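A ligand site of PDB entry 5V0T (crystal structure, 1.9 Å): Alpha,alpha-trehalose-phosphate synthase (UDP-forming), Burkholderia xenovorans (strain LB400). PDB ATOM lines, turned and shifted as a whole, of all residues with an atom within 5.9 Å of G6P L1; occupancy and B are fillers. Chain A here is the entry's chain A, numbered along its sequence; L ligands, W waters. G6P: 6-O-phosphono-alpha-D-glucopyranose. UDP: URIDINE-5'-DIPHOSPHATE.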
ATOM      1  N   ASN A  17     -12.759  19.123  15.081  1.00  0.00           N
ATOM      2  CA  ASN A  17     -11.850  18.098  14.591  1.00  0.00           C
ATOM      3  C   ASN A  17     -10.431  18.396  15.059  1.00  0.00           C
ATOM      4  O   ASN A  17      -9.820  17.607  15.791  1.00  0.00           O
ATOM      5  CB  ASN A  17     -11.896  18.020  13.063  1.00  0.00           C
ATOM      6  CG  ASN A  17     -11.085  16.842  12.543  1.00  0.00           C
ATOM      7  OD1 ASN A  17     -11.393  15.692  12.843  1.00  0.00           O
ATOM      8  ND2 ASN A  17     -10.041  17.129  11.779  1.00  0.00           N
ATOM      9  N   ARG A  18      -9.895  19.532  14.633  1.00  0.00           N
ATOM     10  CA  ARG A  18      -8.542  19.931  15.010  1.00  0.00           C
ATOM     11  C   ARG A  18      -8.549  20.491  16.429  1.00  0.00           C
ATOM     12  O   ARG A  18      -9.369  21.343  16.775  1.00  0.00           O
ATOM     13  CB  ARG A  18      -8.010  20.989  14.036  1.00  0.00           C
ATOM     14  CG  ARG A  18      -6.574  21.470  14.371  1.00  0.00           C
ATOM     15  CD  ARG A  18      -5.585  20.337  14.196  1.00  0.00           C
ATOM     16  NE  ARG A  18      -5.304  20.044  12.791  1.00  0.00           N
ATOM     17  CZ  ARG A  18      -4.620  18.983  12.369  1.00  0.00           C
ATOM     18  NH1 ARG A  18      -4.182  18.087  13.252  1.00  0.00           N
ATOM     19  NH2 ARG A  18      -4.380  18.798  11.074  1.00  0.00           N
ATOM     20  N   ALA A  29      -0.524  25.687  12.040  1.00  0.00           N
ATOM     21  CA  ALA A  29      -1.230  26.726  11.305  1.00  0.00           C
ATOM     22  C   ALA A  29      -2.710  26.381  11.225  1.00  0.00           C
ATOM     23  O   ALA A  29      -3.075  25.239  10.911  1.00  0.00           O
ATOM     24  CB  ALA A  29      -0.640  26.891   9.907  1.00  0.00           C
ATOM     25  N   GLY A  30      -3.561  27.362  11.525  1.00  0.00           N
ATOM     26  CA  GLY A  30      -4.994  27.171  11.440  1.00  0.00           C
ATOM     27  C   GLY A  30      -5.672  28.070  12.453  1.00  0.00           C
ATOM     28  O   GLY A  30      -5.294  28.059  13.626  1.00  0.00           O
ATOM     29  N   GLY A  31      -6.663  28.856  12.011  1.00  0.00           N
ATOM     30  CA  GLY A  31      -7.277  29.837  12.882  1.00  0.00           C
ATOM     31  C   GLY A  31      -8.323  29.282  13.832  1.00  0.00           C
ATOM     32  O   GLY A  31      -8.583  29.878  14.889  1.00  0.00           O
ATOM     33  N   LEU A  32      -8.939  28.161  13.489  1.00  0.00           N
ATOM     34  CA  LEU A  32      -9.867  27.539  14.433  1.00  0.00           C
ATOM     35  C   LEU A  32      -9.168  27.229  15.747  1.00  0.00           C
ATOM     36  O   LEU A  32      -9.626  27.633  16.823  1.00  0.00           O
ATOM     37  CB  LEU A  32     -10.497  26.256  13.832  1.00  0.00           C
ATOM     38  CG  LEU A  32     -11.478  25.487  14.746  1.00  0.00           C
ATOM     39  CD1 LEU A  32     -12.524  24.739  13.937  1.00  0.00           C
ATOM     40  CD2 LEU A  32     -10.782  24.512  15.765  1.00  0.00           C
ATOM     41  N   ALA A  33      -8.035  26.516  15.695  1.00  0.00           N
ATOM     42  CA  ALA A  33      -7.371  26.115  16.922  1.00  0.00           C
ATOM     43  C   ALA A  33      -6.924  27.327  17.720  1.00  0.00           C
ATOM     44  O   ALA A  33      -6.996  27.337  18.958  1.00  0.00           O
ATOM     45  CB  ALA A  33      -6.162  25.209  16.614  1.00  0.00           C
ATOM     46  N   TRP A  50     -10.184  15.334  17.623  1.00  0.00           N
ATOM     47  CA  TRP A  50      -9.155  14.461  17.073  1.00  0.00           C
ATOM     48  C   TRP A  50      -7.794  14.810  17.643  1.00  0.00           C
ATOM     49  O   TRP A  50      -7.437  15.981  17.787  1.00  0.00           O
ATOM     50  CB  TRP A  50      -9.164  14.587  15.538  1.00  0.00           C
ATOM     51  CG  TRP A  50      -8.152  13.800  14.776  1.00  0.00           C
ATOM     52  CD1 TRP A  50      -7.767  12.501  14.988  1.00  0.00           C
ATOM     53  CD2 TRP A  50      -7.410  14.257  13.654  1.00  0.00           C
ATOM     54  NE1 TRP A  50      -6.817  12.125  14.058  1.00  0.00           N
ATOM     55  CE2 TRP A  50      -6.584  13.192  13.222  1.00  0.00           C
ATOM     56  CE3 TRP A  50      -7.352  15.479  12.950  1.00  0.00           C
ATOM     57  CZ2 TRP A  50      -5.728  13.300  12.124  1.00  0.00           C
ATOM     58  CZ3 TRP A  50      -6.496  15.587  11.852  1.00  0.00           C
ATOM     59  CH2 TRP A  50      -5.681  14.501  11.466  1.00  0.00           C
ATOM     60  N   TYR A  86     -12.186  12.739   6.815  1.00  0.00           N
ATOM     61  CA  TYR A  86     -11.367  13.960   6.826  1.00  0.00           C
ATOM     62  C   TYR A  86     -10.780  14.273   5.456  1.00  0.00           C
ATOM     63  O   TYR A  86     -11.095  15.315   4.869  1.00  0.00           O
ATOM     64  CB  TYR A  86     -10.282  13.822   7.896  1.00  0.00           C
ATOM     65  CG  TYR A  86      -9.254  14.937   7.925  1.00  0.00           C
ATOM     66  CD1 TYR A  86      -9.494  16.126   8.614  1.00  0.00           C
ATOM     67  CD2 TYR A  86      -8.028  14.801   7.277  1.00  0.00           C
ATOM     68  CE1 TYR A  86      -8.532  17.152   8.652  1.00  0.00           C
ATOM     69  CE2 TYR A  86      -7.070  15.805   7.309  1.00  0.00           C
ATOM     70  CZ  TYR A  86      -7.331  16.974   8.001  1.00  0.00           C
ATOM     71  OH  TYR A  86      -6.356  17.963   8.023  1.00  0.00           O
ATOM     72  N   ASN A  91     -12.569  17.402   3.344  1.00  0.00           N
ATOM     73  CA  ASN A  91     -11.626  18.265   2.633  1.00  0.00           C
ATOM     74  C   ASN A  91     -11.611  18.086   1.120  1.00  0.00           C
ATOM     75  O   ASN A  91     -11.030  18.924   0.428  1.00  0.00           O
ATOM     76  CB  ASN A  91     -10.235  18.075   3.228  1.00  0.00           C
ATOM     77  CG  ASN A  91     -10.145  18.710   4.590  1.00  0.00           C
ATOM     78  OD1 ASN A  91     -10.874  19.652   4.867  1.00  0.00           O
ATOM     79  ND2 ASN A  91      -9.289  18.197   5.454  1.00  0.00           N
ATOM     80  N   TRP A  95     -14.759  21.428   1.887  1.00  0.00           N
ATOM     81  CA  TRP A  95     -13.830  22.568   1.832  1.00  0.00           C
ATOM     82  C   TRP A  95     -13.821  23.231   0.454  1.00  0.00           C
ATOM     83  O   TRP A  95     -14.016  24.454   0.397  1.00  0.00           O
ATOM     84  CB  TRP A  95     -12.416  22.144   2.245  1.00  0.00           C
ATOM     85  CG  TRP A  95     -11.445  23.310   2.184  1.00  0.00           C
ATOM     86  CD1 TRP A  95     -10.688  23.683   1.117  1.00  0.00           C
ATOM     87  CD2 TRP A  95     -11.158  24.243   3.235  1.00  0.00           C
ATOM     88  NE1 TRP A  95      -9.932  24.792   1.429  1.00  0.00           N
ATOM     89  CE2 TRP A  95     -10.200  25.148   2.724  1.00  0.00           C
ATOM     90  CE3 TRP A  95     -11.588  24.385   4.555  1.00  0.00           C
ATOM     91  CZ2 TRP A  95      -9.672  26.201   3.493  1.00  0.00           C
ATOM     92  CZ3 TRP A  95     -11.053  25.423   5.337  1.00  0.00           C
ATOM     93  CH2 TRP A  95     -10.124  26.329   4.793  1.00  0.00           C
ATOM     94  N   ASP A 140     -17.266  23.727  13.154  1.00  0.00           N
ATOM     95  CA  ASP A 140     -16.774  23.683  11.772  1.00  0.00           C
ATOM     96  C   ASP A 140     -17.267  22.488  10.950  1.00  0.00           C
ATOM     97  O   ASP A 140     -17.946  21.596  11.453  1.00  0.00           O
ATOM     98  CB  ASP A 140     -15.244  23.751  11.702  1.00  0.00           C
ATOM     99  CG  ASP A 140     -14.773  24.761  10.656  1.00  0.00           C
ATOM    100  OD1 ASP A 140     -15.655  25.417  10.061  1.00  0.00           O
ATOM    101  OD2 ASP A 140     -13.551  24.915  10.420  1.00  0.00           O
ATOM    102  N   TYR A 141     -16.918  22.504   9.658  1.00  0.00           N
ATOM    103  CA  TYR A 141     -17.631  21.732   8.646  1.00  0.00           C
ATOM    104  C   TYR A 141     -17.471  20.221   8.804  1.00  0.00           C
ATOM    105  O   TYR A 141     -18.309  19.482   8.269  1.00  0.00           O
ATOM    106  CB  TYR A 141     -17.130  22.162   7.274  1.00  0.00           C
ATOM    107  CG  TYR A 141     -15.626  22.074   7.120  1.00  0.00           C
ATOM    108  CD1 TYR A 141     -14.780  23.082   7.591  1.00  0.00           C
ATOM    109  CD2 TYR A 141     -15.050  21.002   6.467  1.00  0.00           C
ATOM    110  CE1 TYR A 141     -13.400  22.998   7.437  1.00  0.00           C
ATOM    111  CE2 TYR A 141     -13.688  20.912   6.299  1.00  0.00           C
ATOM    112  CZ  TYR A 141     -12.866  21.899   6.789  1.00  0.00           C
ATOM    113  OH  TYR A 141     -11.503  21.788   6.580  1.00  0.00           O
ATOM    114  N   HIS A 142     -16.427  19.738   9.485  1.00  0.00           N
ATOM    115  CA  HIS A 142     -16.264  18.297   9.691  1.00  0.00           C
ATOM    116  C   HIS A 142     -17.423  17.710  10.468  1.00  0.00           C
ATOM    117  O   HIS A 142     -17.713  16.509  10.369  1.00  0.00           O
ATOM    118  CB  HIS A 142     -14.971  17.990  10.453  1.00  0.00           C
ATOM    119  CG  HIS A 142     -13.798  18.782   9.997  1.00  0.00           C
ATOM    120  ND1 HIS A 142     -13.610  20.107  10.349  1.00  0.00           N
ATOM    121  CD2 HIS A 142     -12.742  18.438   9.227  1.00  0.00           C
ATOM    122  CE1 HIS A 142     -12.493  20.547   9.805  1.00  0.00           C
ATOM    123  NE2 HIS A 142     -11.942  19.560   9.119  1.00  0.00           N
ATOM    124  N   HIS A 164     -16.700  27.988  10.786  1.00  0.00           N
ATOM    125  CA  HIS A 164     -15.571  28.924  10.673  1.00  0.00           C
ATOM    126  C   HIS A 164     -15.334  29.333   9.230  1.00  0.00           C
ATOM    127  O   HIS A 164     -14.788  30.405   8.981  1.00  0.00           O
ATOM    128  CB  HIS A 164     -14.287  28.306  11.261  1.00  0.00           C
ATOM    129  CG  HIS A 164     -14.312  28.180  12.751  1.00  0.00           C
ATOM    130  ND1 HIS A 164     -13.506  28.949  13.572  1.00  0.00           N
ATOM    131  CD2 HIS A 164     -15.070  27.426  13.574  1.00  0.00           C
ATOM    132  CE1 HIS A 164     -13.765  28.654  14.838  1.00  0.00           C
ATOM    133  NE2 HIS A 164     -14.712  27.734  14.865  1.00  0.00           N
ATOM    134  N   ILE A 165     -15.726  28.495   8.274  1.00  0.00           N
ATOM    135  CA  ILE A 165     -15.508  28.742   6.846  1.00  0.00           C
ATOM    136  C   ILE A 165     -16.740  29.450   6.289  1.00  0.00           C
ATOM    137  O   ILE A 165     -17.761  29.538   6.989  1.00  0.00           O
ATOM    138  CB  ILE A 165     -15.192  27.423   6.116  1.00  0.00           C
ATOM    139  CG1 ILE A 165     -16.421  26.490   6.122  1.00  0.00           C
ATOM    140  CG2 ILE A 165     -13.968  26.750   6.766  1.00  0.00           C
ATOM    141  CD1 ILE A 165     -16.219  25.231   5.276  1.00  0.00           C
ATOM    142  N   ARG A 277      -1.513  29.198   5.293  1.00  0.00           N
ATOM    143  CA  ARG A 277      -1.458  27.788   4.870  1.00  0.00           C
ATOM    144  C   ARG A 277      -1.460  27.766   3.337  1.00  0.00           C
ATOM    145  O   ARG A 277      -2.124  28.585   2.696  1.00  0.00           O
ATOM    146  CB  ARG A 277      -2.649  27.004   5.423  1.00  0.00           C
ATOM    147  CG  ARG A 277      -2.632  26.736   6.937  1.00  0.00           C
ATOM    148  CD  ARG A 277      -3.857  25.868   7.363  1.00  0.00           C
ATOM    149  NE  ARG A 277      -5.090  26.520   6.916  1.00  0.00           N
ATOM    150  CZ  ARG A 277      -5.795  26.165   5.850  1.00  0.00           C
ATOM    151  NH1 ARG A 277      -5.429  25.113   5.115  1.00  0.00           N
ATOM    152  NH2 ARG A 277      -6.866  26.862   5.520  1.00  0.00           N
ATOM    153  N   THR A 314      -0.019  22.248   4.409  1.00  0.00           N
ATOM    154  CA  THR A 314      -1.321  21.913   4.937  1.00  0.00           C
ATOM    155  C   THR A 314      -1.875  20.754   4.124  1.00  0.00           C
ATOM    156  O   THR A 314      -1.742  20.749   2.895  1.00  0.00           O
ATOM    157  CB  THR A 314      -2.248  23.136   4.899  1.00  0.00           C
ATOM    158  OG1 THR A 314      -3.519  22.800   5.444  1.00  0.00           O
ATOM    159  CG2 THR A 314      -2.430  23.643   3.465  1.00  0.00           C
ATOM    160  N   ARG A 315      -2.453  19.754   4.788  1.00  0.00           N
ATOM    161  CA  ARG A 315      -3.191  18.693   4.094  1.00  0.00           C
ATOM    162  C   ARG A 315      -2.376  18.101   2.936  1.00  0.00           C
ATOM    163  O   ARG A 315      -2.873  17.882   1.828  1.00  0.00           O
ATOM    164  CB  ARG A 315      -4.549  19.221   3.631  1.00  0.00           C
ATOM    165  CG  ARG A 315      -5.418  19.715   4.800  1.00  0.00           C
ATOM    166  CD  ARG A 315      -6.641  20.579   4.383  1.00  0.00           C
ATOM    167  NE  ARG A 315      -7.165  21.324   5.530  1.00  0.00           N
ATOM    168  CZ  ARG A 315      -8.095  22.279   5.457  1.00  0.00           C
ATOM    169  NH1 ARG A 315      -8.636  22.605   4.277  1.00  0.00           N
ATOM    170  NH2 ARG A 315      -8.476  22.907   6.560  1.00  0.00           N
HETATM  171  C1  G6P L   1      -9.254  26.200   8.836  1.00  0.00           C
HETATM  172  C2  G6P L   1     -10.462  25.381   9.246  1.00  0.00           C
HETATM  173  C3  G6P L   1     -10.178  24.616  10.544  1.00  0.00           C
HETATM  174  C4  G6P L   1      -8.912  23.779  10.366  1.00  0.00           C
HETATM  175  C5  G6P L   1      -7.759  24.678   9.930  1.00  0.00           C
HETATM  176  C6  G6P L   1      -6.459  23.875   9.792  1.00  0.00           C
HETATM  177  O1  G6P L   1      -9.018  27.142   9.873  1.00  0.00           O
HETATM  178  O2  G6P L   1     -11.600  26.243   9.389  1.00  0.00           O
HETATM  179  O3  G6P L   1     -11.297  23.759  10.804  1.00  0.00           O
HETATM  180  O4  G6P L   1      -8.555  23.161  11.621  1.00  0.00           O
HETATM  181  O5  G6P L   1      -8.097  25.345   8.706  1.00  0.00           O
HETATM  182  O6  G6P L   1      -6.665  22.770   8.887  1.00  0.00           O
HETATM  183  P   G6P L   1      -6.391  21.269   9.401  1.00  0.00           P
HETATM  184  O1P G6P L   1      -4.897  21.133   9.514  1.00  0.00           O
HETATM  185  O2P G6P L   1      -7.026  20.410   8.347  1.00  0.00           O
HETATM  186  O3P G6P L   1      -7.075  21.185  10.744  1.00  0.00           O
HETATM  187  N1  UDP L   2      -0.274  30.518  12.045  1.00  0.00           N
HETATM  188  C2  UDP L   2       0.719  30.043  12.888  1.00  0.00           C
HETATM  189  N3  UDP L   2       1.869  29.641  12.260  1.00  0.00           N
HETATM  190  C4  UDP L   2       2.119  29.660  10.907  1.00  0.00           C
HETATM  191  C5  UDP L   2       1.044  30.159  10.099  1.00  0.00           C
HETATM  192  C6  UDP L   2      -0.086  30.582  10.678  1.00  0.00           C
HETATM  193  O2  UDP L   2       0.592  29.985  14.089  1.00  0.00           O
HETATM  194  O4  UDP L   2       3.209  29.252  10.492  1.00  0.00           O
HETATM  195  C1' UDP L   2      -1.518  30.980  12.659  1.00  0.00           C
HETATM  196  C2' UDP L   2      -1.818  32.446  12.405  1.00  0.00           C
HETATM  197  O2' UDP L   2      -1.142  33.255  13.366  1.00  0.00           O
HETATM  198  C3' UDP L   2      -3.339  32.471  12.575  1.00  0.00           C
HETATM  199  C4' UDP L   2      -3.758  31.104  12.015  1.00  0.00           C
HETATM  200  O4' UDP L   2      -2.589  30.262  12.086  1.00  0.00           O
HETATM  201  O3' UDP L   2      -3.748  32.562  13.939  1.00  0.00           O
HETATM  202  C5' UDP L   2      -4.280  31.125  10.606  1.00  0.00           C
HETATM  203  O5' UDP L   2      -5.673  31.492  10.675  1.00  0.00           O
HETATM  204  PA  UDP L   2      -6.397  32.185   9.443  1.00  0.00           P
HETATM  205  O1A UDP L   2      -5.567  33.320   8.890  1.00  0.00           O
HETATM  206  O2A UDP L   2      -7.765  32.552   9.912  1.00  0.00           O
HETATM  207  O3A UDP L   2      -6.463  31.089   8.308  1.00  0.00           O
HETATM  208  PB  UDP L   2      -6.719  29.527   8.274  1.00  0.00           P
HETATM  209  O1B UDP L   2      -7.680  29.280   9.439  1.00  0.00           O
HETATM  210  O2B UDP L   2      -7.459  29.335   6.934  1.00  0.00           O
HETATM  211  O3B UDP L   2      -5.453  28.767   8.376  1.00  0.00           O
HETATM  212  O   HOH W   1     -11.182  21.592  12.796  1.00  0.00           O
HETATM  213  O   HOH W   2      -9.396  19.790  11.082  1.00  0.00           O
HETATM  214  O   HOH W   3      -3.466  22.591  11.598  1.00  0.00           O
HETATM  215  O   HOH W   4      -7.294  25.091  13.434  1.00  0.00           O
HETATM  216  O   HOH W   5      -9.638  20.184   7.722  1.00  0.00           O
HETATM  217  O   HOH W   6      -3.143  22.048   8.014  1.00  0.00           O
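Ala 29 touches G6P L1.
Gly 30 touches G6P L1 (CA to C6, 3.97 Å).
N of Gly 31 touches O1 of G6P L1, 3.6 Å away.
Leu 32 touches G6P L1.
Trp 95 touches G6P L1.
CE1 of His 142 touches O3 of G6P L1, 3.6 Å away.
His 164 touches G6P L1 (CB to O2, 3.9 Å).
Ile 165 touches G6P L1 (CG2 to O2, 3.6 Å).
NE of Arg 277 touches O5 of G6P L1, at 3.7 Å.
Hydrophobic or aromatic side chains within 4 Å of G6P L1: Leu 32, Tyr 86, Trp 95, His 142, His 164 and Ile 165.
Within 4 Å of G6P L1: Arg 18, Ala 29, Gly 30, Gly 31, Leu 32, Tyr 86, Trp 95, Asp 140, His 142, His 164, Ile 165, Arg 277 and Arg 315.
An oxygen (O2P) of G6P L1 lies within hydrogen-bond range of the side-chain hydroxyl of Tyr 86.
The side-chain carboxylate of Asp 140 lies within hydrogen-bond range of an oxygen (O3) of G6P L1 (2.6 Å).
NH2 of Arg 18 is in salt-bridge range of O1P of G6P L1 (2.9 Å).
NE of Arg 315 is in salt-bridge range of O2P of G6P L1 (3.0 Å).
N of Gly 31 is in hydrogen-bond range of O1B of UDP L2, at 2.8 Å.
O3B of UDP L2 lies within salt-bridge range of NE of Arg 277 (2.7 Å).
An oxygen (O4') of UDP L2 is in hydrogen-bond range of the backbone NH (N) of Gly 30, at 3.1 Å.
O1B of UDP L2 is in hydrogen-bond range of O1 of G6P L1 (2.6 Å).
Water W6 bridges O1P of G6P L1 and OG1 of Thr 314.
Water W5 lies within hydrogen-bond range of O2P of G6P L1 (2.7 Å), OH of Tyr 141 (2.7 Å), NE2 of His 142 (2.8 Å), ND2 of Asn 91 (3.0 Å) and NH2 of Arg 315 (3.2 Å).
Water W2 lies within hydrogen-bond range of an oxygen (O3P) of G6P L1 (2.7 Å), the side-chain amide nitrogen of Asn 17 (2.8 Å) and a ring nitrogen (NE2) of His 142 (3.2 Å).
Water W3 lies within hydrogen-bond range of O of Ala 29 (2.8 Å), O1P of G6P L1 (2.9 Å) and NE of Arg 18 (3.4 Å).
Water W4 lies within hydrogen-bond range of N of Ala 33, O4 of G6P L1 and N of Leu 32.
Water W1 bridges O3 of G6P L1 (2.9 Å) and N of Arg 18 (3.0 Å).
The backbone carbonyl oxygen (O) of Tyr 86 lies within hydrogen-bond range of the backbone NH (N) of Asn 91 (3.0 Å).
The backbone NH of His 164 is in hydrogen-bond range of the side-chain carboxylate of Asp 140, 2.9 Å away.
The guanidinium group of Arg 315 is in hydrogen-bond range of the side-chain hydroxyl of Tyr 141 (3.2 Å).
A ring nitrogen (NE2) of His 142 is in hydrogen-bond range of the side-chain hydroxyl of Tyr 141, at 3.4 Å.
The guanidinium group (NH1) of Arg 277 is in hydrogen-bond range of the side-chain hydroxyl (OG1) of Thr 314 (3.0 Å).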
